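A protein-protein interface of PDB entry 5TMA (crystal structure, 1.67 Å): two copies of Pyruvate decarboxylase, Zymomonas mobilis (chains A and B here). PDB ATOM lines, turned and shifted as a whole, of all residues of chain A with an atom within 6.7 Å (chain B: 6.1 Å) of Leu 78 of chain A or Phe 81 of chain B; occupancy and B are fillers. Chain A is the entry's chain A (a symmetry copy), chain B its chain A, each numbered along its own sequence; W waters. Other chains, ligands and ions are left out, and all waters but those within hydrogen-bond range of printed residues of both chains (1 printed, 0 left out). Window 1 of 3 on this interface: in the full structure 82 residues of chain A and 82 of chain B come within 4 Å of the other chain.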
ATOM      1  N   GLU A  50      -6.428 -24.356  -7.981  1.00  0.00           N
ATOM      2  CA  GLU A  50      -7.680 -24.876  -7.526  1.00  0.00           C
ATOM      3  C   GLU A  50      -8.782 -24.973  -8.570  1.00  0.00           C
ATOM      4  O   GLU A  50      -9.597 -25.923  -8.488  1.00  0.00           O
ATOM      5  CB  GLU A  50      -8.191 -24.115  -6.311  1.00  0.00           C
ATOM      6  CG  GLU A  50      -7.282 -24.348  -5.093  1.00  0.00           C
ATOM      7  CD  GLU A  50      -6.137 -23.329  -5.002  1.00  0.00           C
ATOM      8  OE1 GLU A  50      -5.935 -22.480  -5.995  1.00  0.00           O
ATOM      9  OE2 GLU A  50      -5.440 -23.404  -3.888  1.00  0.00           O
ATOM     10  N   VAL A  71      -9.370 -28.414  -1.032  1.00  0.00           N
ATOM     11  CA  VAL A  71      -8.820 -27.124  -1.215  1.00  0.00           C
ATOM     12  C   VAL A  71      -8.778 -26.381   0.102  1.00  0.00           C
ATOM     13  O   VAL A  71      -9.376 -26.801   1.084  1.00  0.00           O
ATOM     14  CB  VAL A  71      -9.647 -26.268  -2.290  1.00  0.00           C
ATOM     15  CG1 VAL A  71      -9.687 -26.986  -3.576  1.00  0.00           C
ATOM     16  CG2 VAL A  71     -11.007 -25.984  -1.812  1.00  0.00           C
ATOM     17  N   THR A  72      -8.026 -25.264   0.139  1.00  0.00           N
ATOM     18  CA  THR A  72      -7.947 -24.381   1.308  1.00  0.00           C
ATOM     19  C   THR A  72      -9.000 -23.256   1.282  1.00  0.00           C
ATOM     20  O   THR A  72      -9.514 -22.821   0.263  1.00  0.00           O
ATOM     21  CB  THR A  72      -6.526 -23.785   1.665  1.00  0.00           C
ATOM     22  OG1 THR A  72      -6.464 -23.535   3.110  1.00  0.00           O
ATOM     23  CG2 THR A  72      -6.217 -22.483   0.802  1.00  0.00           C
ATOM     24  N   TYR A  73      -9.323 -22.822   2.465  1.00  0.00           N
ATOM     25  CA  TYR A  73     -10.401 -21.865   2.724  1.00  0.00           C
ATOM     26  C   TYR A  73     -10.242 -20.589   1.919  1.00  0.00           C
ATOM     27  O   TYR A  73      -9.165 -20.049   1.801  1.00  0.00           O
ATOM     28  CB  TYR A  73     -10.443 -21.540   4.204  1.00  0.00           C
ATOM     29  CG  TYR A  73     -11.663 -20.775   4.632  1.00  0.00           C
ATOM     30  CD1 TYR A  73     -12.910 -21.376   4.646  1.00  0.00           C
ATOM     31  CD2 TYR A  73     -11.573 -19.437   4.956  1.00  0.00           C
ATOM     32  CE1 TYR A  73     -14.054 -20.697   4.969  1.00  0.00           C
ATOM     33  CE2 TYR A  73     -12.755 -18.677   5.264  1.00  0.00           C
ATOM     34  CZ  TYR A  73     -13.964 -19.309   5.262  1.00  0.00           C
ATOM     35  OH  TYR A  73     -15.100 -18.607   5.576  1.00  0.00           O
ATOM     36  N   SER A  74     -11.307 -20.284   1.202  1.00  0.00           N
ATOM     37  CA  SER A  74     -11.503 -19.012   0.553  1.00  0.00           C
ATOM     38  C   SER A  74     -10.666 -18.792  -0.699  1.00  0.00           C
ATOM     39  O   SER A  74     -11.191 -18.809  -1.853  1.00  0.00           O
ATOM     40  CB  SER A  74     -11.419 -17.885   1.587  1.00  0.00           C
ATOM     41  OG  SER A  74     -11.892 -16.670   1.079  1.00  0.00           O
ATOM     42  N   VAL A  75      -9.353 -18.646  -0.546  1.00  0.00           N
ATOM     43  CA  VAL A  75      -8.485 -18.565  -1.732  1.00  0.00           C
ATOM     44  C   VAL A  75      -8.531 -19.839  -2.618  1.00  0.00           C
ATOM     45  O   VAL A  75      -8.337 -19.797  -3.811  1.00  0.00           O
ATOM     46  CB  VAL A  75      -7.035 -18.191  -1.337  1.00  0.00           C
ATOM     47  CG1 VAL A  75      -7.054 -16.848  -0.684  1.00  0.00           C
ATOM     48  CG2 VAL A  75      -6.404 -19.217  -0.398  1.00  0.00           C
ATOM     49  N   GLY A  76      -8.691 -21.014  -2.022  1.00  0.00           N
ATOM     50  CA  GLY A  76      -8.786 -22.214  -2.846  1.00  0.00           C
ATOM     51  C   GLY A  76     -10.201 -22.470  -3.288  1.00  0.00           C
ATOM     52  O   GLY A  76     -10.463 -22.811  -4.421  1.00  0.00           O
ATOM     53  N   ALA A  77     -11.124 -22.396  -2.367  1.00  0.00           N
ATOM     54  CA  ALA A  77     -12.459 -22.763  -2.632  1.00  0.00           C
ATOM     55  C   ALA A  77     -13.160 -21.863  -3.664  1.00  0.00           C
ATOM     56  O   ALA A  77     -13.908 -22.343  -4.489  1.00  0.00           O
ATOM     57  CB  ALA A  77     -13.235 -22.768  -1.336  1.00  0.00           C
ATOM     58  N   LEU A  78     -12.962 -20.572  -3.605  1.00  0.00           N
ATOM     59  CA  LEU A  78     -13.769 -19.693  -4.497  1.00  0.00           C
ATOM     60  C   LEU A  78     -13.527 -19.938  -5.974  1.00  0.00           C
ATOM     61  O   LEU A  78     -14.461 -19.996  -6.785  1.00  0.00           O
ATOM     62  CB  LEU A  78     -13.641 -18.232  -4.116  1.00  0.00           C
ATOM     63  CG  LEU A  78     -14.675 -17.693  -3.127  1.00  0.00           C
ATOM     64  CD1 LEU A  78     -14.760 -18.442  -1.833  1.00  0.00           C
ATOM     65  CD2 LEU A  78     -14.444 -16.215  -2.823  1.00  0.00           C
ATOM     66  N   SER A  79     -12.281 -20.155  -6.379  1.00  0.00           N
ATOM     67  CA  SER A  79     -12.007 -20.508  -7.779  1.00  0.00           C
ATOM     68  C   SER A  79     -12.548 -21.912  -8.073  1.00  0.00           C
ATOM     69  O   SER A  79     -13.221 -22.192  -9.144  1.00  0.00           O
ATOM     70  CB  SER A  79     -10.504 -20.401  -8.117  1.00  0.00           C
ATOM     71  OG  SER A  79      -9.730 -21.139  -7.181  1.00  0.00           O
ATOM     72  N   ALA A  80     -12.341 -22.831  -7.131  1.00  0.00           N
ATOM     73  CA  ALA A  80     -12.851 -24.226  -7.334  1.00  0.00           C
ATOM     74  C   ALA A  80     -14.374 -24.248  -7.543  1.00  0.00           C
ATOM     75  O   ALA A  80     -14.847 -25.101  -8.262  1.00  0.00           O
ATOM     76  CB  ALA A  80     -12.482 -25.173  -6.222  1.00  0.00           C
ATOM     77  N   PHE A  81     -15.069 -23.240  -7.024  1.00  0.00           N
ATOM     78  CA  PHE A  81     -16.519 -23.146  -7.261  1.00  0.00           C
ATOM     79  C   PHE A  81     -16.880 -23.112  -8.727  1.00  0.00           C
ATOM     80  O   PHE A  81     -17.986 -23.573  -9.118  1.00  0.00           O
ATOM     81  CB  PHE A  81     -17.150 -21.945  -6.555  1.00  0.00           C
ATOM     82  CG  PHE A  81     -17.228 -22.047  -5.046  1.00  0.00           C
ATOM     83  CD1 PHE A  81     -17.124 -23.241  -4.334  1.00  0.00           C
ATOM     84  CD2 PHE A  81     -17.536 -20.891  -4.348  1.00  0.00           C
ATOM     85  CE1 PHE A  81     -17.267 -23.263  -2.980  1.00  0.00           C
ATOM     86  CE2 PHE A  81     -17.764 -20.929  -2.937  1.00  0.00           C
ATOM     87  CZ  PHE A  81     -17.552 -22.127  -2.280  1.00  0.00           C
ATOM     88  N   ASP A  82     -16.038 -22.474  -9.521  1.00  0.00           N
ATOM     89  CA  ASP A  82     -16.256 -22.455 -10.974  1.00  0.00           C
ATOM     90  C   ASP A  82     -16.361 -23.921 -11.507  1.00  0.00           C
ATOM     91  O   ASP A  82     -17.332 -24.326 -12.224  1.00  0.00           O
ATOM     92  CB  ASP A  82     -15.252 -21.574 -11.628  1.00  0.00           C
ATOM     93  CG  ASP A  82     -15.612 -21.163 -13.047  1.00  0.00           C
ATOM     94  OD1 ASP A  82     -16.390 -21.854 -13.732  1.00  0.00           O
ATOM     95  OD2 ASP A  82     -15.113 -20.083 -13.467  1.00  0.00           O
ATOM     96  N   ALA A  83     -15.386 -24.767 -11.136  1.00  0.00           N
ATOM     97  CA  ALA A  83     -15.424 -26.154 -11.512  1.00  0.00           C
ATOM     98  C   ALA A  83     -16.580 -26.955 -10.934  1.00  0.00           C
ATOM     99  O   ALA A  83     -17.138 -27.845 -11.585  1.00  0.00           O
ATOM    100  CB  ALA A  83     -14.101 -26.808 -11.183  1.00  0.00           C
ATOM    101  N   LEU A  96     -16.558 -31.487  -3.093  1.00  0.00           N
ATOM    102  CA  LEU A  96     -15.588 -30.473  -2.767  1.00  0.00           C
ATOM    103  C   LEU A  96     -15.462 -30.413  -1.258  1.00  0.00           C
ATOM    104  O   LEU A  96     -16.434 -30.114  -0.571  1.00  0.00           O
ATOM    105  CB  LEU A  96     -15.963 -29.070  -3.295  1.00  0.00           C
ATOM    106  CG  LEU A  96     -14.943 -27.936  -3.050  1.00  0.00           C
ATOM    107  CD1 LEU A  96     -13.646 -28.211  -3.800  1.00  0.00           C
ATOM    108  CD2 LEU A  96     -15.560 -26.589  -3.459  1.00  0.00           C
ATOM    109  N   LEU A 116     -12.083 -12.259   4.116  1.00  0.00           N
ATOM    110  CA  LEU A 116     -12.400 -10.915   3.616  1.00  0.00           C
ATOM    111  C   LEU A 116     -11.938  -9.758   4.459  1.00  0.00           C
ATOM    112  O   LEU A 116     -12.047  -8.582   4.066  1.00  0.00           O
ATOM    113  CB  LEU A 116     -13.899 -10.753   3.400  1.00  0.00           C
ATOM    114  CG  LEU A 116     -14.496 -11.730   2.420  1.00  0.00           C
ATOM    115  CD1 LEU A 116     -16.021 -11.784   2.468  1.00  0.00           C
ATOM    116  CD2 LEU A 116     -14.035 -11.380   0.998  1.00  0.00           C
ATOM    117  N   TYR A 123     -19.587 -16.968   4.789  1.00  0.00           N
ATOM    118  CA  TYR A 123     -19.804 -16.561   3.384  1.00  0.00           C
ATOM    119  C   TYR A 123     -19.518 -17.645   2.349  1.00  0.00           C
ATOM    120  O   TYR A 123     -20.235 -17.812   1.364  1.00  0.00           O
ATOM    121  CB  TYR A 123     -19.059 -15.325   3.027  1.00  0.00           C
ATOM    122  CG  TYR A 123     -17.584 -15.434   2.997  1.00  0.00           C
ATOM    123  CD1 TYR A 123     -16.877 -15.747   1.865  1.00  0.00           C
ATOM    124  CD2 TYR A 123     -16.899 -15.091   4.133  1.00  0.00           C
ATOM    125  CE1 TYR A 123     -15.457 -15.843   1.924  1.00  0.00           C
ATOM    126  CE2 TYR A 123     -15.573 -15.171   4.199  1.00  0.00           C
ATOM    127  CZ  TYR A 123     -14.836 -15.509   3.092  1.00  0.00           C
ATOM    128  OH  TYR A 123     -13.449 -15.510   3.167  1.00  0.00           O
ATOM    129  N   GLN A 124     -18.473 -18.449   2.642  1.00  0.00           N
ATOM    130  CA  GLN A 124     -18.099 -19.523   1.697  1.00  0.00           C
ATOM    131  C   GLN A 124     -19.160 -20.587   1.611  1.00  0.00           C
ATOM    132  O   GLN A 124     -19.538 -20.984   0.495  1.00  0.00           O
ATOM    133  CB  GLN A 124     -16.717 -20.052   2.061  1.00  0.00           C
ATOM    134  CG  GLN A 124     -16.265 -21.078   1.069  1.00  0.00           C
ATOM    135  CD  GLN A 124     -14.860 -21.506   1.326  1.00  0.00           C
ATOM    136  OE1 GLN A 124     -13.943 -20.754   1.080  1.00  0.00           O
ATOM    137  NE2 GLN A 124     -14.666 -22.762   1.760  1.00  0.00           N
ATOM    138  N   MET A 127     -22.123 -19.190  -0.365  1.00  0.00           N
ATOM    139  CA  MET A 127     -21.847 -19.198  -1.776  1.00  0.00           C
ATOM    140  C   MET A 127     -21.999 -20.593  -2.329  1.00  0.00           C
ATOM    141  O   MET A 127     -22.641 -20.792  -3.380  1.00  0.00           O
ATOM    142  CB  MET A 127     -20.437 -18.611  -2.054  1.00  0.00           C
ATOM    143  CG  MET A 127     -20.355 -17.131  -1.745  1.00  0.00           C
ATOM    144  SD  MET A 127     -18.703 -16.525  -1.918  1.00  0.00           S
ATOM    145  CE  MET A 127     -18.478 -16.360  -3.699  1.00  0.00           C
ATOM    146  N   GLY B  76     -16.971 -17.389 -16.469  1.00  0.00           N
ATOM    147  CA  GLY B  76     -15.947 -16.380 -16.226  1.00  0.00           C
ATOM    148  C   GLY B  76     -16.049 -15.812 -14.835  1.00  0.00           C
ATOM    149  O   GLY B  76     -15.068 -15.619 -14.152  1.00  0.00           O
ATOM    150  N   ALA B  77     -17.241 -15.454 -14.436  1.00  0.00           N
ATOM    151  CA  ALA B  77     -17.434 -14.774 -13.217  1.00  0.00           C
ATOM    152  C   ALA B  77     -17.069 -15.605 -11.975  1.00  0.00           C
ATOM    153  O   ALA B  77     -16.509 -15.086 -11.033  1.00  0.00           O
ATOM    154  CB  ALA B  77     -18.871 -14.315 -13.131  1.00  0.00           C
ATOM    155  N   LEU B  78     -17.411 -16.867 -11.944  1.00  0.00           N
ATOM    156  CA  LEU B  78     -17.204 -17.622 -10.677  1.00  0.00           C
ATOM    157  C   LEU B  78     -15.750 -17.725 -10.259  1.00  0.00           C
ATOM    158  O   LEU B  78     -15.397 -17.548  -9.085  1.00  0.00           O
ATOM    159  CB  LEU B  78     -17.904 -18.967 -10.701  1.00  0.00           C
ATOM    160  CG  LEU B  78     -19.331 -19.002 -10.153  1.00  0.00           C
ATOM    161  CD1 LEU B  78     -20.279 -18.041 -10.801  1.00  0.00           C
ATOM    162  CD2 LEU B  78     -19.928 -20.405 -10.229  1.00  0.00           C
ATOM    163  N   SER B  79     -14.841 -17.949 -11.201  1.00  0.00           N
ATOM    164  CA  SER B  79     -13.410 -17.946 -10.865  1.00  0.00           C
ATOM    165  C   SER B  79     -12.966 -16.521 -10.511  1.00  0.00           C
ATOM    166  O   SER B  79     -12.219 -16.256  -9.485  1.00  0.00           O
ATOM    167  CB  SER B  79     -12.550 -18.536 -12.004  1.00  0.00           C
ATOM    168  OG  SER B  79     -12.848 -17.896 -13.237  1.00  0.00           O
ATOM    169  N   ALA B  80     -13.443 -15.546 -11.284  1.00  0.00           N
ATOM    170  CA  ALA B  80     -13.069 -14.124 -10.995  1.00  0.00           C
ATOM    171  C   ALA B  80     -13.485 -13.705  -9.576  1.00  0.00           C
ATOM    172  O   ALA B  80     -12.801 -12.896  -8.988  1.00  0.00           O
ATOM    173  CB  ALA B  80     -13.622 -13.139 -11.993  1.00  0.00           C
ATOM    174  N   PHE B  81     -14.501 -14.363  -9.026  1.00  0.00           N
ATOM    175  CA  PHE B  81     -14.897 -14.079  -7.636  1.00  0.00           C
ATOM    176  C   PHE B  81     -13.771 -14.269  -6.649  1.00  0.00           C
ATOM    177  O   PHE B  81     -13.737 -13.589  -5.588  1.00  0.00           O
ATOM    178  CB  PHE B  81     -16.107 -14.903  -7.193  1.00  0.00           C
ATOM    179  CG  PHE B  81     -17.425 -14.515  -7.830  1.00  0.00           C
ATOM    180  CD1 PHE B  81     -17.663 -13.294  -8.458  1.00  0.00           C
ATOM    181  CD2 PHE B  81     -18.486 -15.391  -7.673  1.00  0.00           C
ATOM    182  CE1 PHE B  81     -18.895 -12.990  -8.954  1.00  0.00           C
ATOM    183  CE2 PHE B  81     -19.796 -15.038  -8.123  1.00  0.00           C
ATOM    184  CZ  PHE B  81     -19.943 -13.853  -8.821  1.00  0.00           C
ATOM    185  N   ASP B  82     -12.927 -15.252  -6.907  1.00  0.00           N
ATOM    186  CA  ASP B  82     -11.751 -15.467  -6.053  1.00  0.00           C
ATOM    187  C   ASP B  82     -10.909 -14.152  -5.980  1.00  0.00           C
ATOM    188  O   ASP B  82     -10.553 -13.622  -4.879  1.00  0.00           O
ATOM    189  CB  ASP B  82     -11.034 -16.701  -6.473  1.00  0.00           C
ATOM    190  CG  ASP B  82     -10.058 -17.238  -5.439  1.00  0.00           C
ATOM    191  OD1 ASP B  82      -9.571 -16.488  -4.572  1.00  0.00           O
ATOM    192  OD2 ASP B  82      -9.802 -18.473  -5.490  1.00  0.00           O
ATOM    193  N   ALA B  83     -10.603 -13.569  -7.151  1.00  0.00           N
ATOM    194  CA  ALA B  83      -9.894 -12.320  -7.194  1.00  0.00           C
ATOM    195  C   ALA B  83     -10.629 -11.132  -6.592  1.00  0.00           C
ATOM    196  O   ALA B  83     -10.027 -10.250  -5.968  1.00  0.00           O
ATOM    197  CB  ALA B  83      -9.470 -12.023  -8.614  1.00  0.00           C
ATOM    198  N   ILE B  84     -11.960 -11.100  -6.788  1.00  0.00           N
ATOM    199  CA  ILE B  84     -12.770 -10.050  -6.224  1.00  0.00           C
ATOM    200  C   ILE B  84     -12.829 -10.099  -4.693  1.00  0.00           C
ATOM    201  O   ILE B  84     -12.703  -9.079  -4.055  1.00  0.00           O
ATOM    202  CB  ILE B  84     -14.198 -10.044  -6.804  1.00  0.00           C
ATOM    203  CG1 ILE B  84     -14.144  -9.673  -8.250  1.00  0.00           C
ATOM    204  CG2 ILE B  84     -15.177  -9.167  -6.049  1.00  0.00           C
ATOM    205  CD1 ILE B  84     -13.430  -8.436  -8.580  1.00  0.00           C
ATOM    206  N   GLY B  85     -12.982 -11.282  -4.092  1.00  0.00           N
ATOM    207  CA  GLY B  85     -12.833 -11.477  -2.695  1.00  0.00           C
ATOM    208  C   GLY B  85     -11.428 -11.014  -2.282  1.00  0.00           C
ATOM    209  O   GLY B  85     -11.304 -10.315  -1.244  1.00  0.00           O
ATOM    210  N   GLY B  86     -10.404 -11.267  -3.122  1.00  0.00           N
ATOM    211  CA  GLY B  86      -9.086 -10.695  -2.849  1.00  0.00           C
ATOM    212  C   GLY B  86      -9.080  -9.161  -2.786  1.00  0.00           C
ATOM    213  O   GLY B  86      -8.426  -8.561  -1.903  1.00  0.00           O
ATOM    214  N   LEU B  96     -16.162  -5.471 -10.989  1.00  0.00           N
ATOM    215  CA  LEU B  96     -16.352  -6.644 -11.803  1.00  0.00           C
ATOM    216  C   LEU B  96     -17.635  -6.468 -12.589  1.00  0.00           C
ATOM    217  O   LEU B  96     -18.706  -6.349 -12.000  1.00  0.00           O
ATOM    218  CB  LEU B  96     -16.441  -7.953 -10.985  1.00  0.00           C
ATOM    219  CG  LEU B  96     -16.576  -9.268 -11.784  1.00  0.00           C
ATOM    220  CD1 LEU B  96     -15.328  -9.514 -12.623  1.00  0.00           C
ATOM    221  CD2 LEU B  96     -16.848 -10.432 -10.819  1.00  0.00           C
ATOM    222  N   TYR B 123     -28.391 -16.866  -9.343  1.00  0.00           N
ATOM    223  CA  TYR B 123     -27.369 -17.438  -8.440  1.00  0.00           C
ATOM    224  C   TYR B 123     -26.043 -16.684  -8.413  1.00  0.00           C
ATOM    225  O   TYR B 123     -25.420 -16.498  -7.369  1.00  0.00           O
ATOM    226  CB  TYR B 123     -27.115 -18.877  -8.707  1.00  0.00           C
ATOM    227  CG  TYR B 123     -26.473 -19.203 -10.000  1.00  0.00           C
ATOM    228  CD1 TYR B 123     -25.115 -19.313 -10.157  1.00  0.00           C
ATOM    229  CD2 TYR B 123     -27.290 -19.519 -11.053  1.00  0.00           C
ATOM    230  CE1 TYR B 123     -24.576 -19.617 -11.440  1.00  0.00           C
ATOM    231  CE2 TYR B 123     -26.799 -19.810 -12.254  1.00  0.00           C
ATOM    232  CZ  TYR B 123     -25.444 -19.900 -12.453  1.00  0.00           C
ATOM    233  OH  TYR B 123     -24.959 -20.283 -13.697  1.00  0.00           O
ATOM    234  N   GLN B 124     -25.653 -16.173  -9.601  1.00  0.00           N
ATOM    235  CA  GLN B 124     -24.373 -15.438  -9.689  1.00  0.00           C
ATOM    236  C   GLN B 124     -24.415 -14.148  -8.915  1.00  0.00           C
ATOM    237  O   GLN B 124     -23.478 -13.865  -8.148  1.00  0.00           O
ATOM    238  CB  GLN B 124     -23.991 -15.270 -11.155  1.00  0.00           C
ATOM    239  CG  GLN B 124     -22.653 -14.610 -11.281  1.00  0.00           C
ATOM    240  CD  GLN B 124     -22.198 -14.563 -12.700  1.00  0.00           C
ATOM    241  OE1 GLN B 124     -21.835 -15.577 -13.253  1.00  0.00           O
ATOM    242  NE2 GLN B 124     -22.140 -13.359 -13.291  1.00  0.00           N
ATOM    243  N   LEU B 125     -25.472 -13.355  -9.095  1.00  0.00           N
ATOM    244  CA  LEU B 125     -25.660 -12.149  -8.315  1.00  0.00           C
ATOM    245  C   LEU B 125     -25.678 -12.477  -6.778  1.00  0.00           C
ATOM    246  O   LEU B 125     -25.041 -11.778  -5.993  1.00  0.00           O
ATOM    247  CB  LEU B 125     -26.958 -11.475  -8.741  1.00  0.00           C
ATOM    248  CG  LEU B 125     -27.368 -10.289  -7.937  1.00  0.00           C
ATOM    249  CD1 LEU B 125     -26.429  -9.149  -8.125  1.00  0.00           C
ATOM    250  CD2 LEU B 125     -28.798  -9.843  -8.336  1.00  0.00           C
ATOM    251  N   MET B 127     -24.266 -14.968  -5.181  1.00  0.00           N
ATOM    252  CA  MET B 127     -22.924 -15.292  -4.781  1.00  0.00           C
ATOM    253  C   MET B 127     -22.103 -14.034  -4.646  1.00  0.00           C
ATOM    254  O   MET B 127     -21.384 -13.851  -3.642  1.00  0.00           O
ATOM    255  CB  MET B 127     -22.290 -16.298  -5.779  1.00  0.00           C
ATOM    256  CG  MET B 127     -22.950 -17.659  -5.727  1.00  0.00           C
ATOM    257  SD  MET B 127     -22.317 -18.733  -6.981  1.00  0.00           S
ATOM    258  CE  MET B 127     -20.722 -19.271  -6.337  1.00  0.00           C
ATOM    259  N   ALA B 128     -22.257 -13.112  -5.612  1.00  0.00           N
ATOM    260  CA  ALA B 128     -21.473 -11.882  -5.623  1.00  0.00           C
ATOM    261  C   ALA B 128     -21.669 -11.010  -4.422  1.00  0.00           C
ATOM    262  O   ALA B 128     -20.710 -10.319  -3.916  1.00  0.00           O
ATOM    263  CB  ALA B 128     -21.683 -11.056  -6.902  1.00  0.00           C
ATOM    264  N   ILE B 131     -19.178 -10.994  -1.358  1.00  0.00           N
ATOM    265  CA  ILE B 131     -17.790 -10.633  -1.485  1.00  0.00           C
ATOM    266  C   ILE B 131     -17.595  -9.256  -2.112  1.00  0.00           C
ATOM    267  O   ILE B 131     -16.499  -8.906  -2.563  1.00  0.00           O
ATOM    268  CB  ILE B 131     -16.996 -11.666  -2.307  1.00  0.00           C
ATOM    269  CG1 ILE B 131     -17.604 -11.807  -3.703  1.00  0.00           C
ATOM    270  CG2 ILE B 131     -16.910 -12.997  -1.586  1.00  0.00           C
ATOM    271  CD1 ILE B 131     -16.828 -12.625  -4.695  1.00  0.00           C
ATOM    272  N   TYR B 163     -19.912  -5.385  -7.964  1.00  0.00           N
ATOM    273  CA  TYR B 163     -20.337  -6.278  -9.027  1.00  0.00           C
ATOM    274  C   TYR B 163     -21.448  -5.633  -9.880  1.00  0.00           C
ATOM    275  O   TYR B 163     -22.402  -5.084  -9.360  1.00  0.00           O
ATOM    276  CB  TYR B 163     -20.803  -7.582  -8.423  1.00  0.00           C
ATOM    277  CG  TYR B 163     -21.533  -8.550  -9.366  1.00  0.00           C
ATOM    278  CD1 TYR B 163     -22.905  -8.512  -9.555  1.00  0.00           C
ATOM    279  CD2 TYR B 163     -20.817  -9.508 -10.092  1.00  0.00           C
ATOM    280  CE1 TYR B 163     -23.515  -9.406 -10.399  1.00  0.00           C
ATOM    281  CE2 TYR B 163     -21.434 -10.417 -10.882  1.00  0.00           C
ATOM    282  CZ  TYR B 163     -22.774 -10.371 -11.051  1.00  0.00           C
ATOM    283  OH  TYR B 163     -23.404 -11.320 -11.822  1.00  0.00           O
ATOM    284  N   TRP B 412      -5.491 -11.488   1.851  1.00  0.00           N
ATOM    285  CA  TRP B 412      -6.057 -12.573   1.096  1.00  0.00           C
ATOM    286  C   TRP B 412      -5.065 -13.736   0.971  1.00  0.00           C
ATOM    287  O   TRP B 412      -5.380 -14.901   1.189  1.00  0.00           O
ATOM    288  CB  TRP B 412      -6.458 -12.050  -0.265  1.00  0.00           C
ATOM    289  CG  TRP B 412      -7.447 -12.886  -1.017  1.00  0.00           C
ATOM    290  CD1 TRP B 412      -7.281 -13.402  -2.307  1.00  0.00           C
ATOM    291  CD2 TRP B 412      -8.762 -13.279  -0.602  1.00  0.00           C
ATOM    292  NE1 TRP B 412      -8.432 -14.067  -2.690  1.00  0.00           N
ATOM    293  CE2 TRP B 412      -9.362 -13.992  -1.676  1.00  0.00           C
ATOM    294  CE3 TRP B 412      -9.521 -13.095   0.571  1.00  0.00           C
ATOM    295  CZ2 TRP B 412     -10.663 -14.502  -1.602  1.00  0.00           C
ATOM    296  CZ3 TRP B 412     -10.853 -13.546   0.599  1.00  0.00           C
ATOM    297  CH2 TRP B 412     -11.412 -14.239  -0.502  1.00  0.00           C
HETATM  298  O   HOH W   1     -16.731 -18.403  -6.810  1.00  0.00           O
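OD2 of Asp 82 of chain A lies within hydrogen-bond range of N of Ser 79 of chain B, 3.1 Å away.
O of Val 75 of chain A lies close to OD2 of Asp 82 of chain B (2.6 Å).
The backbone NH (N) of Ser 79 of chain A lies within hydrogen-bond range of the side-chain carboxylate (OD2) of Asp 82 of chain B.
O of Leu 78 of chain A lies close to O of Leu 78 of chain B, at 3.5 Å.
OG of Ser 79 of chain B is in hydrogen-bond range of O of Gly 76 of chain B (3.3 Å).
The indole nitrogen of Trp 412 of chain B is in hydrogen-bond range of the backbone carbonyl oxygen of Asp 82 of chain B, 3.1 Å away.
OG of Ser 74 of chain A is in hydrogen-bond range of OH of Tyr 123 of chain A (2.9 Å).
The backbone NH of Ser 74 of chain A is in hydrogen-bond range of the side-chain amide oxygen of Gln 124 of chain A (2.7 Å).
The side-chain hydroxyl (OG) of Ser 79 of chain A lies within hydrogen-bond range of the backbone carbonyl oxygen (O) of Gly 76 of chain A, 3.3 Å away.
Ser 74 of chain A touches Trp 412 of chain B (OG to CH2, 2.9 Å).
CG1 of Val 75 of chain A touches O of Trp 412 of chain B, at 3.2 Å.
CD2 of Leu 78 of chain A touches O of Phe 81 of chain B, 3.9 Å away.
CB of Leu 78 of chain A touches CB of Asp 82 of chain B, 3.8 Å away.
O of Phe 81 of chain A touches CD2 of Leu 78 of chain B, at 3.9 Å.
Asp 82 of chain A touches Leu 78 of chain B (CB to CB, 3.8 Å).
Gly 85 of chain B touches Leu 116 of chain A.
CZ3 of Trp 412 of chain B touches CD2 of Leu 116 of chain A (3.9 Å).
CE of Met 127 of chain B touches O of Met 127 of chain A (3.8 Å).
Met 127 of chain A touches Ile 131 of chain B.
Leu 78 of chain A touches just these residues of chain B: Leu 78 (3.5 Å), Phe 81 (3.9 Å) and Asp 82 (3.8 Å).
Of chain A, only Leu 78 (3.9 Å) comes within 4 Å of Phe 81 of chain B.
Of the printed residues of chain B, Leu 116 of chain A touches Gly 85 (3.7 Å) and Trp 412 (3.9 Å).
Printed residues of chain B within 4 Å of Met 127 of chain A: Met 127 and Ile 131.
The nearest residue of chain A that does not touch Phe 81 of chain B is Met 127 of chain A (4.1 Å).
Hydrophobic or aromatic side chains of chain A within 4 Å of the printed part of chain B: Val 75, Leu 78, Leu 116 and Met 127.
Hydrophobic or aromatic side chains of chain B that line the printed part of chain A: Leu 78, Met 127, Ile 131 and Trp 412.
Among the printed residues, no Asp or Glu carboxylate lies within 4 Å of a Lys or Arg side-chain nitrogen of the other chain.
Leu 78 of chain A touches its own counterpart, Leu 78 of chain B.
Leu 78 of chain A touches Phe 81 of chain B, and with the chains exchanged Phe 81 of chain A touches Leu 78 of chain B.
Leu 78 of chain A touches Asp 82 of chain B, and with the chains exchanged Asp 82 of chain A touches Leu 78 of chain B.
Met 127 of chain B touches its own counterpart, Met 127 of chain A.
Of the 15 pairs that touch across the chains among the printed residues, 8 have their exchanged pair printed and touching as well.
Water W1 lies within hydrogen-bond range of the backbone carbonyl oxygen of Leu 78 of chain B (2.8 Å) and the backbone carbonyl oxygen of Leu 78 of chain A (2.8 Å).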
